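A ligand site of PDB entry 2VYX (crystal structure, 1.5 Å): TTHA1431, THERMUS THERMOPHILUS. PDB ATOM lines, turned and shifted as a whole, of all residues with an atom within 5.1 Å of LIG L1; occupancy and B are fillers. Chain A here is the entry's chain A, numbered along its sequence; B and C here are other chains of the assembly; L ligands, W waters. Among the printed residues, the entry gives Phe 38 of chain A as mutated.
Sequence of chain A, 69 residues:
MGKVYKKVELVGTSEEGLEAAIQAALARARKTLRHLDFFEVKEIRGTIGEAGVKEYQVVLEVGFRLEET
O of Tyr 5 is in hydrogen-bond range of N of Val 11 of chain C (2.7 Å).
The backbone carbonyl oxygen (O) of Lys 3 lies within hydrogen-bond range of the side-chain hydroxyl (OG1) of Thr 13 of chain C.
The guanidinium group (NH2) of Arg 45 of chain B is in salt-bridge range of the side-chain carboxylate (OE2) of Glu 40 (2.9 Å).
O of His 35 sits at hydrogen-bond distance from N of Arg 65, 3.1 Å away.
The backbone carbonyl oxygen (O) of Gln 57 of chain C sits at hydrogen-bond distance from the backbone NH (N) of Arg 45 of chain C (2.8 Å).
The backbone carbonyl oxygen (O) of Arg 45 of chain B is in hydrogen-bond range of the backbone NH (N) of Gln 57 of chain B (2.8 Å).
CD of Lys 3 touches O8 of LIG L1, 3.9 Å away.
CZ of Phe 38 touches C6 of LIG L1, at 3.4 Å.
CG2 of Thr 47 of chain B touches O1 of LIG L1, at 2.8 Å.
CG1 of Val 11 of chain C touches C7 of LIG L1 (3.8 Å).
Arg 45 of chain C touches LIG L1.
Gln 57 of chain C touches LIG L1.
11 residues have an atom within 4 Å of LIG L1: Lys 3, Tyr 5, Asp 37, Phe 38, Arg 65, Arg 45 of chain B, Thr 47 of chain B, Gln 57 of chain B, Val 11 of chain C, Arg 45 of chain C and Gln 57 of chain C.
OE1 of Gln 57 of chain C sits at hydrogen-bond distance from N2 of LG2 L2, at 2.7 Å.
The backbone carbonyl oxygen (O) of Asp 37 sits at hydrogen-bond distance from an oxygen (O3) of LIG L1, at 3.5 Å.
The side-chain carboxylate (OD2) of Asp 37 lies close to an oxygen (O9) of LIG L1, at 2.7 Å.
NH1 of Arg 65 lies within salt-bridge range of O9 of LIG L1 (3.4 Å).
The guanidinium group (NE) of Arg 45 of chain B sits at hydrogen-bond distance from an oxygen (O2) of LIG L1.
NE of Arg 45 of chain C sits at hydrogen-bond distance from O2 of LG2 L2 (2.7 Å).
A nitrogen (N2) of LIG L1 sits at hydrogen-bond distance from the side-chain amide oxygen of Gln 57 of chain B (2.8 Å).
O8 of LIG L1 sits at hydrogen-bond distance from OH of Tyr 5, 2.7 Å away.
Water W4 bridges O of Asp 37 (2.6 Å) and O3 of LIG L1 (3.0 Å).
Water W1 lies within hydrogen-bond range of an oxygen (O4) of LG2 L2 and an oxygen (O4) of LIG L1.
Water W2 lies within hydrogen-bond range of OH of Tyr 5 and O5 of LIG L1.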
ATOM      1  N   LYS A   3     -19.824 -10.928   4.016  1.00  0.00           N
ATOM      2  CA  LYS A   3     -18.463 -11.461   4.096  1.00  0.00           C
ATOM      3  C   LYS A   3     -17.846 -11.692   2.730  1.00  0.00           C
ATOM      4  O   LYS A   3     -18.539 -11.943   1.738  1.00  0.00           O
ATOM      5  CB  LYS A   3     -18.384 -12.731   4.961  1.00  0.00           C
ATOM      6  CG  LYS A   3     -19.369 -13.824   4.657  1.00  0.00           C
ATOM      7  CD  LYS A   3     -19.360 -14.862   5.778  1.00  0.00           C
ATOM      8  CE  LYS A   3     -20.689 -15.547   5.919  1.00  0.00           C
ATOM      9  NZ  LYS A   3     -21.761 -14.574   6.286  1.00  0.00           N
ATOM     10  N   TYR A   5     -14.351 -13.515   0.771  1.00  0.00           N
ATOM     11  CA  TYR A   5     -13.244 -14.458   0.825  1.00  0.00           C
ATOM     12  C   TYR A   5     -12.259 -14.163  -0.282  1.00  0.00           C
ATOM     13  O   TYR A   5     -12.630 -13.620  -1.326  1.00  0.00           O
ATOM     14  CB  TYR A   5     -13.751 -15.897   0.676  1.00  0.00           C
ATOM     15  CG  TYR A   5     -14.758 -16.298   1.730  1.00  0.00           C
ATOM     16  CD1 TYR A   5     -16.081 -15.889   1.634  1.00  0.00           C
ATOM     17  CD2 TYR A   5     -14.392 -17.075   2.825  1.00  0.00           C
ATOM     18  CE1 TYR A   5     -17.002 -16.241   2.597  1.00  0.00           C
ATOM     19  CE2 TYR A   5     -15.302 -17.431   3.780  1.00  0.00           C
ATOM     20  CZ  TYR A   5     -16.613 -16.999   3.663  1.00  0.00           C
ATOM     21  OH  TYR A   5     -17.530 -17.344   4.630  1.00  0.00           O
ATOM     22  N   HIS A  35      -7.928 -17.701   9.089  1.00  0.00           N
ATOM     23  CA  HIS A  35      -9.282 -18.009   8.594  1.00  0.00           C
ATOM     24  C   HIS A  35      -9.246 -18.759   7.255  1.00  0.00           C
ATOM     25  O   HIS A  35     -10.085 -18.541   6.393  1.00  0.00           O
ATOM     26  CB  HIS A  35     -10.149 -16.757   8.497  1.00  0.00           C
ATOM     27  CG  HIS A  35     -10.025 -15.834   9.663  1.00  0.00           C
ATOM     28  ND1 HIS A  35     -10.414 -16.200  10.937  1.00  0.00           N
ATOM     29  CD2 HIS A  35      -9.539 -14.570   9.769  1.00  0.00           C
ATOM     30  CE1 HIS A  35     -10.176 -15.192  11.767  1.00  0.00           C
ATOM     31  NE2 HIS A  35      -9.652 -14.190  11.080  1.00  0.00           N
ATOM     32  N   ASP A  37     -10.138 -21.663   5.041  1.00  0.00           N
ATOM     33  CA  ASP A  37     -11.399 -22.388   5.107  1.00  0.00           C
ATOM     34  C   ASP A  37     -11.447 -23.616   4.206  1.00  0.00           C
ATOM     35  O   ASP A  37     -11.788 -24.710   4.653  1.00  0.00           O
ATOM     36  CB  ASP A  37     -12.564 -21.449   4.774  1.00  0.00           C
ATOM     37  CG  ASP A  37     -12.937 -20.531   5.924  1.00  0.00           C
ATOM     38  OD1 ASP A  37     -12.737 -20.929   7.092  1.00  0.00           O
ATOM     39  OD2 ASP A  37     -13.427 -19.415   5.669  1.00  0.00           O
ATOM     40  N   PHE A  38     -11.121 -23.422   2.928  1.00  0.00           N
ATOM     41  CA  PHE A  38     -11.281 -24.502   1.956  1.00  0.00           C
ATOM     42  C   PHE A  38     -10.188 -24.496   0.910  1.00  0.00           C
ATOM     43  O   PHE A  38      -9.500 -23.476   0.716  1.00  0.00           O
ATOM     44  CB  PHE A  38     -12.657 -24.420   1.279  1.00  0.00           C
ATOM     45  CG  PHE A  38     -12.881 -23.144   0.497  1.00  0.00           C
ATOM     46  CD1 PHE A  38     -13.434 -22.032   1.109  1.00  0.00           C
ATOM     47  CD2 PHE A  38     -12.547 -23.071  -0.847  1.00  0.00           C
ATOM     48  CE1 PHE A  38     -13.633 -20.863   0.417  1.00  0.00           C
ATOM     49  CE2 PHE A  38     -12.745 -21.889  -1.557  1.00  0.00           C
ATOM     50  CZ  PHE A  38     -13.294 -20.783  -0.921  1.00  0.00           C
ATOM     51  N   PHE A  39     -10.001 -25.626   0.237  1.00  0.00           N
ATOM     52  CA  PHE A  39      -9.114 -25.724  -0.905  1.00  0.00           C
ATOM     53  C   PHE A  39      -9.754 -26.507  -2.065  1.00  0.00           C
ATOM     54  O   PHE A  39     -10.701 -27.273  -1.868  1.00  0.00           O
ATOM     55  CB  PHE A  39      -7.782 -26.342  -0.518  1.00  0.00           C
ATOM     56  CG  PHE A  39      -7.857 -27.791  -0.108  1.00  0.00           C
ATOM     57  CD1 PHE A  39      -7.665 -28.795  -1.039  1.00  0.00           C
ATOM     58  CD2 PHE A  39      -8.101 -28.139   1.223  1.00  0.00           C
ATOM     59  CE1 PHE A  39      -7.748 -30.123  -0.658  1.00  0.00           C
ATOM     60  CE2 PHE A  39      -8.175 -29.444   1.605  1.00  0.00           C
ATOM     61  CZ  PHE A  39      -7.993 -30.458   0.677  1.00  0.00           C
ATOM     62  N   GLU A  40      -9.202 -26.293  -3.256  1.00  0.00           N
ATOM     63  CA  GLU A  40      -9.639 -26.972  -4.487  1.00  0.00           C
ATOM     64  C   GLU A  40      -8.391 -27.331  -5.251  1.00  0.00           C
ATOM     65  O   GLU A  40      -7.578 -26.470  -5.526  1.00  0.00           O
ATOM     66  CB  GLU A  40     -10.476 -26.031  -5.364  1.00  0.00           C
ATOM     67  CG  GLU A  40     -11.746 -25.482  -4.740  1.00  0.00           C
ATOM     68  CD  GLU A  40     -12.203 -24.133  -5.339  1.00  0.00           C
ATOM     69  OE1 GLU A  40     -11.628 -23.659  -6.347  1.00  0.00           O
ATOM     70  OE2 GLU A  40     -13.147 -23.548  -4.749  1.00  0.00           O
ATOM     71  N   ARG A  65     -11.328 -16.349   4.608  1.00  0.00           N
ATOM     72  CA  ARG A  65     -12.216 -15.223   4.879  1.00  0.00           C
ATOM     73  C   ARG A  65     -11.390 -13.987   5.205  1.00  0.00           C
ATOM     74  O   ARG A  65     -10.501 -14.035   6.051  1.00  0.00           O
ATOM     75  CB  ARG A  65     -13.150 -15.528   6.042  1.00  0.00           C
ATOM     76  CG  ARG A  65     -14.270 -14.508   6.190  1.00  0.00           C
ATOM     77  CD  ARG A  65     -15.005 -14.632   7.513  1.00  0.00           C
ATOM     78  NE  ARG A  65     -14.305 -13.917   8.582  1.00  0.00           N
ATOM     79  CZ  ARG A  65     -13.569 -14.480   9.543  1.00  0.00           C
ATOM     80  NH1 ARG A  65     -13.403 -15.809   9.635  1.00  0.00           N
ATOM     81  NH2 ARG A  65     -12.984 -13.693  10.451  1.00  0.00           N
ATOM     82  N   ARG B  45     -11.468 -31.511  -3.468  1.00  0.00           N
ATOM     83  CA  ARG B  45     -11.739 -30.333  -2.675  1.00  0.00           C
ATOM     84  C   ARG B  45     -11.439 -30.698  -1.230  1.00  0.00           C
ATOM     85  O   ARG B  45     -11.133 -31.842  -0.925  1.00  0.00           O
ATOM     86  CB  ARG B  45     -13.219 -29.932  -2.771  1.00  0.00           C
ATOM     87  CG  ARG B  45     -13.776 -29.699  -4.148  1.00  0.00           C
ATOM     88  CD  ARG B  45     -15.183 -29.075  -4.086  1.00  0.00           C
ATOM     89  NE  ARG B  45     -15.114 -27.689  -3.634  1.00  0.00           N
ATOM     90  CZ  ARG B  45     -15.321 -26.614  -4.390  1.00  0.00           C
ATOM     91  NH1 ARG B  45     -15.628 -26.718  -5.676  1.00  0.00           N
ATOM     92  NH2 ARG B  45     -15.201 -25.408  -3.839  1.00  0.00           N
ATOM     93  N   GLY B  46     -11.546 -29.725  -0.327  1.00  0.00           N
ATOM     94  CA  GLY B  46     -11.474 -30.031   1.085  1.00  0.00           C
ATOM     95  C   GLY B  46     -11.571 -28.838   2.006  1.00  0.00           C
ATOM     96  O   GLY B  46     -11.698 -27.700   1.564  1.00  0.00           O
ATOM     97  N   THR B  47     -11.547 -29.126   3.294  1.00  0.00           N
ATOM     98  CA  THR B  47     -11.620 -28.097   4.319  1.00  0.00           C
ATOM     99  C   THR B  47     -10.256 -28.015   4.993  1.00  0.00           C
ATOM    100  O   THR B  47      -9.473 -28.950   4.969  1.00  0.00           O
ATOM    101  CB  THR B  47     -12.697 -28.410   5.372  1.00  0.00           C
ATOM    102  OG1 THR B  47     -12.531 -29.755   5.825  1.00  0.00           O
ATOM    103  CG2 THR B  47     -14.107 -28.247   4.781  1.00  0.00           C
ATOM    104  N   GLN B  57     -12.329 -34.120   0.281  1.00  0.00           N
ATOM    105  CA  GLN B  57     -13.652 -34.309  -0.319  1.00  0.00           C
ATOM    106  C   GLN B  57     -13.466 -34.594  -1.805  1.00  0.00           C
ATOM    107  O   GLN B  57     -13.073 -33.730  -2.565  1.00  0.00           O
ATOM    108  CB  GLN B  57     -14.497 -33.073  -0.115  1.00  0.00           C
ATOM    109  CG  GLN B  57     -14.689 -32.738   1.352  1.00  0.00           C
ATOM    110  CD  GLN B  57     -15.194 -31.340   1.577  1.00  0.00           C
ATOM    111  OE1 GLN B  57     -15.127 -30.509   0.676  1.00  0.00           O
ATOM    112  NE2 GLN B  57     -15.754 -31.090   2.765  1.00  0.00           N
ATOM    113  N   VAL C  11     -14.324 -13.829  -3.461  1.00  0.00           N
ATOM    114  CA  VAL C  11     -15.642 -14.403  -3.355  1.00  0.00           C
ATOM    115  C   VAL C  11     -16.521 -13.449  -2.553  1.00  0.00           C
ATOM    116  O   VAL C  11     -16.330 -13.290  -1.352  1.00  0.00           O
ATOM    117  CB  VAL C  11     -15.642 -15.769  -2.650  1.00  0.00           C
ATOM    118  CG1 VAL C  11     -17.010 -16.416  -2.762  1.00  0.00           C
ATOM    119  CG2 VAL C  11     -14.579 -16.682  -3.235  1.00  0.00           C
ATOM    120  N   THR C  13     -20.188 -12.497  -0.923  1.00  0.00           N
ATOM    121  CA  THR C  13     -21.373 -13.176  -0.422  1.00  0.00           C
ATOM    122  C   THR C  13     -22.478 -12.196  -0.069  1.00  0.00           C
ATOM    123  O   THR C  13     -22.224 -11.029   0.262  1.00  0.00           O
ATOM    124  CB  THR C  13     -21.088 -14.112   0.783  1.00  0.00           C
ATOM    125  OG1 THR C  13     -20.854 -13.347   1.980  1.00  0.00           O
ATOM    126  CG2 THR C  13     -19.879 -15.026   0.508  1.00  0.00           C
ATOM    127  N   ARG C  45     -22.073 -19.983  -6.678  1.00  0.00           N
ATOM    128  CA  ARG C  45     -22.297 -21.045  -5.708  1.00  0.00           C
ATOM    129  C   ARG C  45     -23.181 -20.491  -4.590  1.00  0.00           C
ATOM    130  O   ARG C  45     -23.643 -19.337  -4.615  1.00  0.00           O
ATOM    131  CB  ARG C  45     -20.963 -21.543  -5.131  1.00  0.00           C
ATOM    132  CG  ARG C  45     -19.854 -21.851  -6.123  1.00  0.00           C
ATOM    133  CD  ARG C  45     -18.571 -22.282  -5.427  1.00  0.00           C
ATOM    134  NE  ARG C  45     -18.753 -23.545  -4.703  1.00  0.00           N
ATOM    135  CZ  ARG C  45     -18.606 -24.768  -5.220  1.00  0.00           C
ATOM    136  NH1 ARG C  45     -18.238 -24.955  -6.481  1.00  0.00           N
ATOM    137  NH2 ARG C  45     -18.837 -25.827  -4.454  1.00  0.00           N
ATOM    138  N   GLN C  57     -22.980 -16.915  -3.237  1.00  0.00           N
ATOM    139  CA  GLN C  57     -21.532 -16.812  -3.188  1.00  0.00           C
ATOM    140  C   GLN C  57     -21.009 -16.725  -4.608  1.00  0.00           C
ATOM    141  O   GLN C  57     -21.003 -17.723  -5.358  1.00  0.00           O
ATOM    142  CB  GLN C  57     -20.922 -18.006  -2.463  1.00  0.00           C
ATOM    143  CG  GLN C  57     -21.363 -18.161  -1.003  1.00  0.00           C
ATOM    144  CD  GLN C  57     -21.006 -19.515  -0.410  1.00  0.00           C
ATOM    145  OE1 GLN C  57     -20.615 -20.436  -1.137  1.00  0.00           O
ATOM    146  NE2 GLN C  57     -21.127 -19.645   0.902  1.00  0.00           N
ATOM    147  N   VAL C  59     -17.996 -16.095  -7.120  1.00  0.00           N
ATOM    148  CA  VAL C  59     -16.550 -16.133  -7.292  1.00  0.00           C
ATOM    149  C   VAL C  59     -16.224 -15.262  -8.486  1.00  0.00           C
ATOM    150  O   VAL C  59     -16.739 -15.487  -9.580  1.00  0.00           O
ATOM    151  CB  VAL C  59     -16.031 -17.577  -7.529  1.00  0.00           C
ATOM    152  CG1 VAL C  59     -14.504 -17.559  -7.531  1.00  0.00           C
ATOM    153  CG2 VAL C  59     -16.594 -18.531  -6.463  1.00  0.00           C
HETATM  154  N1  LIG L   1     -16.710 -26.076   2.583  1.00  0.00           N
HETATM  155  C1  LIG L   1     -16.384 -27.402   2.355  1.00  0.00           C
HETATM  156  O1  LIG L   1     -16.494 -28.219   3.264  1.00  0.00           O
HETATM  157  N2  LIG L   1     -15.965 -27.826   1.111  1.00  0.00           N
HETATM  158  C2  LIG L   1     -15.868 -26.926   0.073  1.00  0.00           C
HETATM  159  O2  LIG L   1     -15.191 -27.254  -0.908  1.00  0.00           O
HETATM  160  C3  LIG L   1     -16.193 -25.587   0.284  1.00  0.00           C
HETATM  161  N3  LIG L   1     -16.103 -24.680  -0.755  1.00  0.00           N
HETATM  162  C4  LIG L   1     -16.425 -23.352  -0.534  1.00  0.00           C
HETATM  163  C5  LIG L   1     -16.329 -22.455  -1.586  1.00  0.00           C
HETATM  164  C6  LIG L   1     -16.649 -21.103  -1.415  1.00  0.00           C
HETATM  165  C7  LIG L   1     -16.868 -20.225  -2.597  1.00  0.00           C
HETATM  166  C8  LIG L   1     -17.050 -20.669  -0.146  1.00  0.00           C
HETATM  167  C9  LIG L   1     -17.267 -19.198   0.075  1.00  0.00           C
HETATM  168  C10 LIG L   1     -17.168 -21.559   0.920  1.00  0.00           C
HETATM  169  C11 LIG L   1     -16.849 -22.914   0.736  1.00  0.00           C
HETATM  170  N4  LIG L   1     -16.941 -23.837   1.779  1.00  0.00           N
HETATM  171  C12 LIG L   1     -16.613 -25.176   1.546  1.00  0.00           C
HETATM  172  C13 LIG L   1     -17.327 -23.456   3.177  1.00  0.00           C
HETATM  173  C14 LIG L   1     -16.106 -22.846   3.865  1.00  0.00           C
HETATM  174  O3  LIG L   1     -15.108 -23.810   4.056  1.00  0.00           O
HETATM  175  C15 LIG L   1     -16.449 -22.249   5.214  1.00  0.00           C
HETATM  176  O4  LIG L   1     -16.887 -23.278   6.076  1.00  0.00           O
HETATM  177  C16 LIG L   1     -17.531 -21.184   5.114  1.00  0.00           C
HETATM  178  O5  LIG L   1     -17.245 -20.239   4.094  1.00  0.00           O
HETATM  179  C17 LIG L   1     -17.607 -20.424   6.424  1.00  0.00           C
HETATM  180  O6  LIG L   1     -16.347 -19.842   6.575  1.00  0.00           O
HETATM  181  P1  LIG L   1     -16.125 -18.693   7.665  1.00  0.00           P
HETATM  182  O7  LIG L   1     -16.628 -19.217   8.986  1.00  0.00           O
HETATM  183  O8  LIG L   1     -16.914 -17.502   7.204  1.00  0.00           O
HETATM  184  O9  LIG L   1     -14.660 -18.327   7.765  1.00  0.00           O
HETATM  185  N1  LG2 L   2     -20.162 -24.535   1.622  1.00  0.00           N
HETATM  186  C1  LG2 L   2     -20.363 -23.276   1.142  1.00  0.00           C
HETATM  187  O1  LG2 L   2     -20.669 -22.377   1.903  1.00  0.00           O
HETATM  188  N2  LG2 L   2     -20.245 -22.993  -0.207  1.00  0.00           N
HETATM  189  C2  LG2 L   2     -19.877 -23.990  -1.081  1.00  0.00           C
HETATM  190  O2  LG2 L   2     -19.915 -23.718  -2.276  1.00  0.00           O
HETATM  191  C3  LG2 L   2     -19.651 -25.299  -0.620  1.00  0.00           C
HETATM  192  N3  LG2 L   2     -19.303 -26.329  -1.470  1.00  0.00           N
HETATM  193  C4  LG2 L   2     -19.085 -27.595  -0.959  1.00  0.00           C
HETATM  194  C5  LG2 L   2     -18.713 -28.631  -1.824  1.00  0.00           C
HETATM  195  C6  LG2 L   2     -18.505 -29.924  -1.329  1.00  0.00           C
HETATM  196  C7  LG2 L   2     -17.877 -30.954  -2.215  1.00  0.00           C
HETATM  197  C8  LG2 L   2     -18.674 -30.173   0.030  1.00  0.00           C
HETATM  198  C9  LG2 L   2     -18.764 -31.597   0.502  1.00  0.00           C
HETATM  199  C10 LG2 L   2     -19.027 -29.146   0.889  1.00  0.00           C
HETATM  200  C11 LG2 L   2     -19.235 -27.850   0.407  1.00  0.00           C
HETATM  201  N4  LG2 L   2     -19.603 -26.814   1.250  1.00  0.00           N
HETATM  202  C12 LG2 L   2     -19.818 -25.558   0.749  1.00  0.00           C
HETATM  203  C13 LG2 L   2     -19.942 -27.037   2.711  1.00  0.00           C
HETATM  204  C14 LG2 L   2     -21.330 -27.667   2.844  1.00  0.00           C
HETATM  205  O3  LG2 L   2     -22.333 -26.756   2.439  1.00  0.00           O
HETATM  206  C15 LG2 L   2     -21.621 -28.107   4.281  1.00  0.00           C
HETATM  207  O4  LG2 L   2     -21.621 -26.946   5.086  1.00  0.00           O
HETATM  208  C16 LG2 L   2     -20.618 -29.114   4.826  1.00  0.00           C
HETATM  209  O5  LG2 L   2     -20.451 -30.171   3.910  1.00  0.00           O
HETATM  210  C17 LG2 L   2     -21.095 -29.685   6.142  1.00  0.00           C
HETATM  211  O6  LG2 L   2     -22.356 -30.231   5.850  1.00  0.00           O
HETATM  212  P1  LG2 L   2     -23.115 -31.249   6.816  1.00  0.00           P
HETATM  213  O7  LG2 L   2     -22.159 -32.379   7.088  1.00  0.00           O
HETATM  214  O8  LG2 L   2     -23.522 -30.528   8.074  1.00  0.00           O
HETATM  215  O9  LG2 L   2     -24.349 -31.686   6.094  1.00  0.00           O
HETATM  216  O   HOH W   1     -19.406 -25.623   5.959  1.00  0.00           O
HETATM  217  O   HOH W   2     -20.197 -18.433   4.211  1.00  0.00           O
HETATM  218  O   HOH W   3     -17.355 -27.379   5.559  1.00  0.00           O
HETATM  219  O   HOH W   4     -13.666 -24.714   6.476  1.00  0.00           O
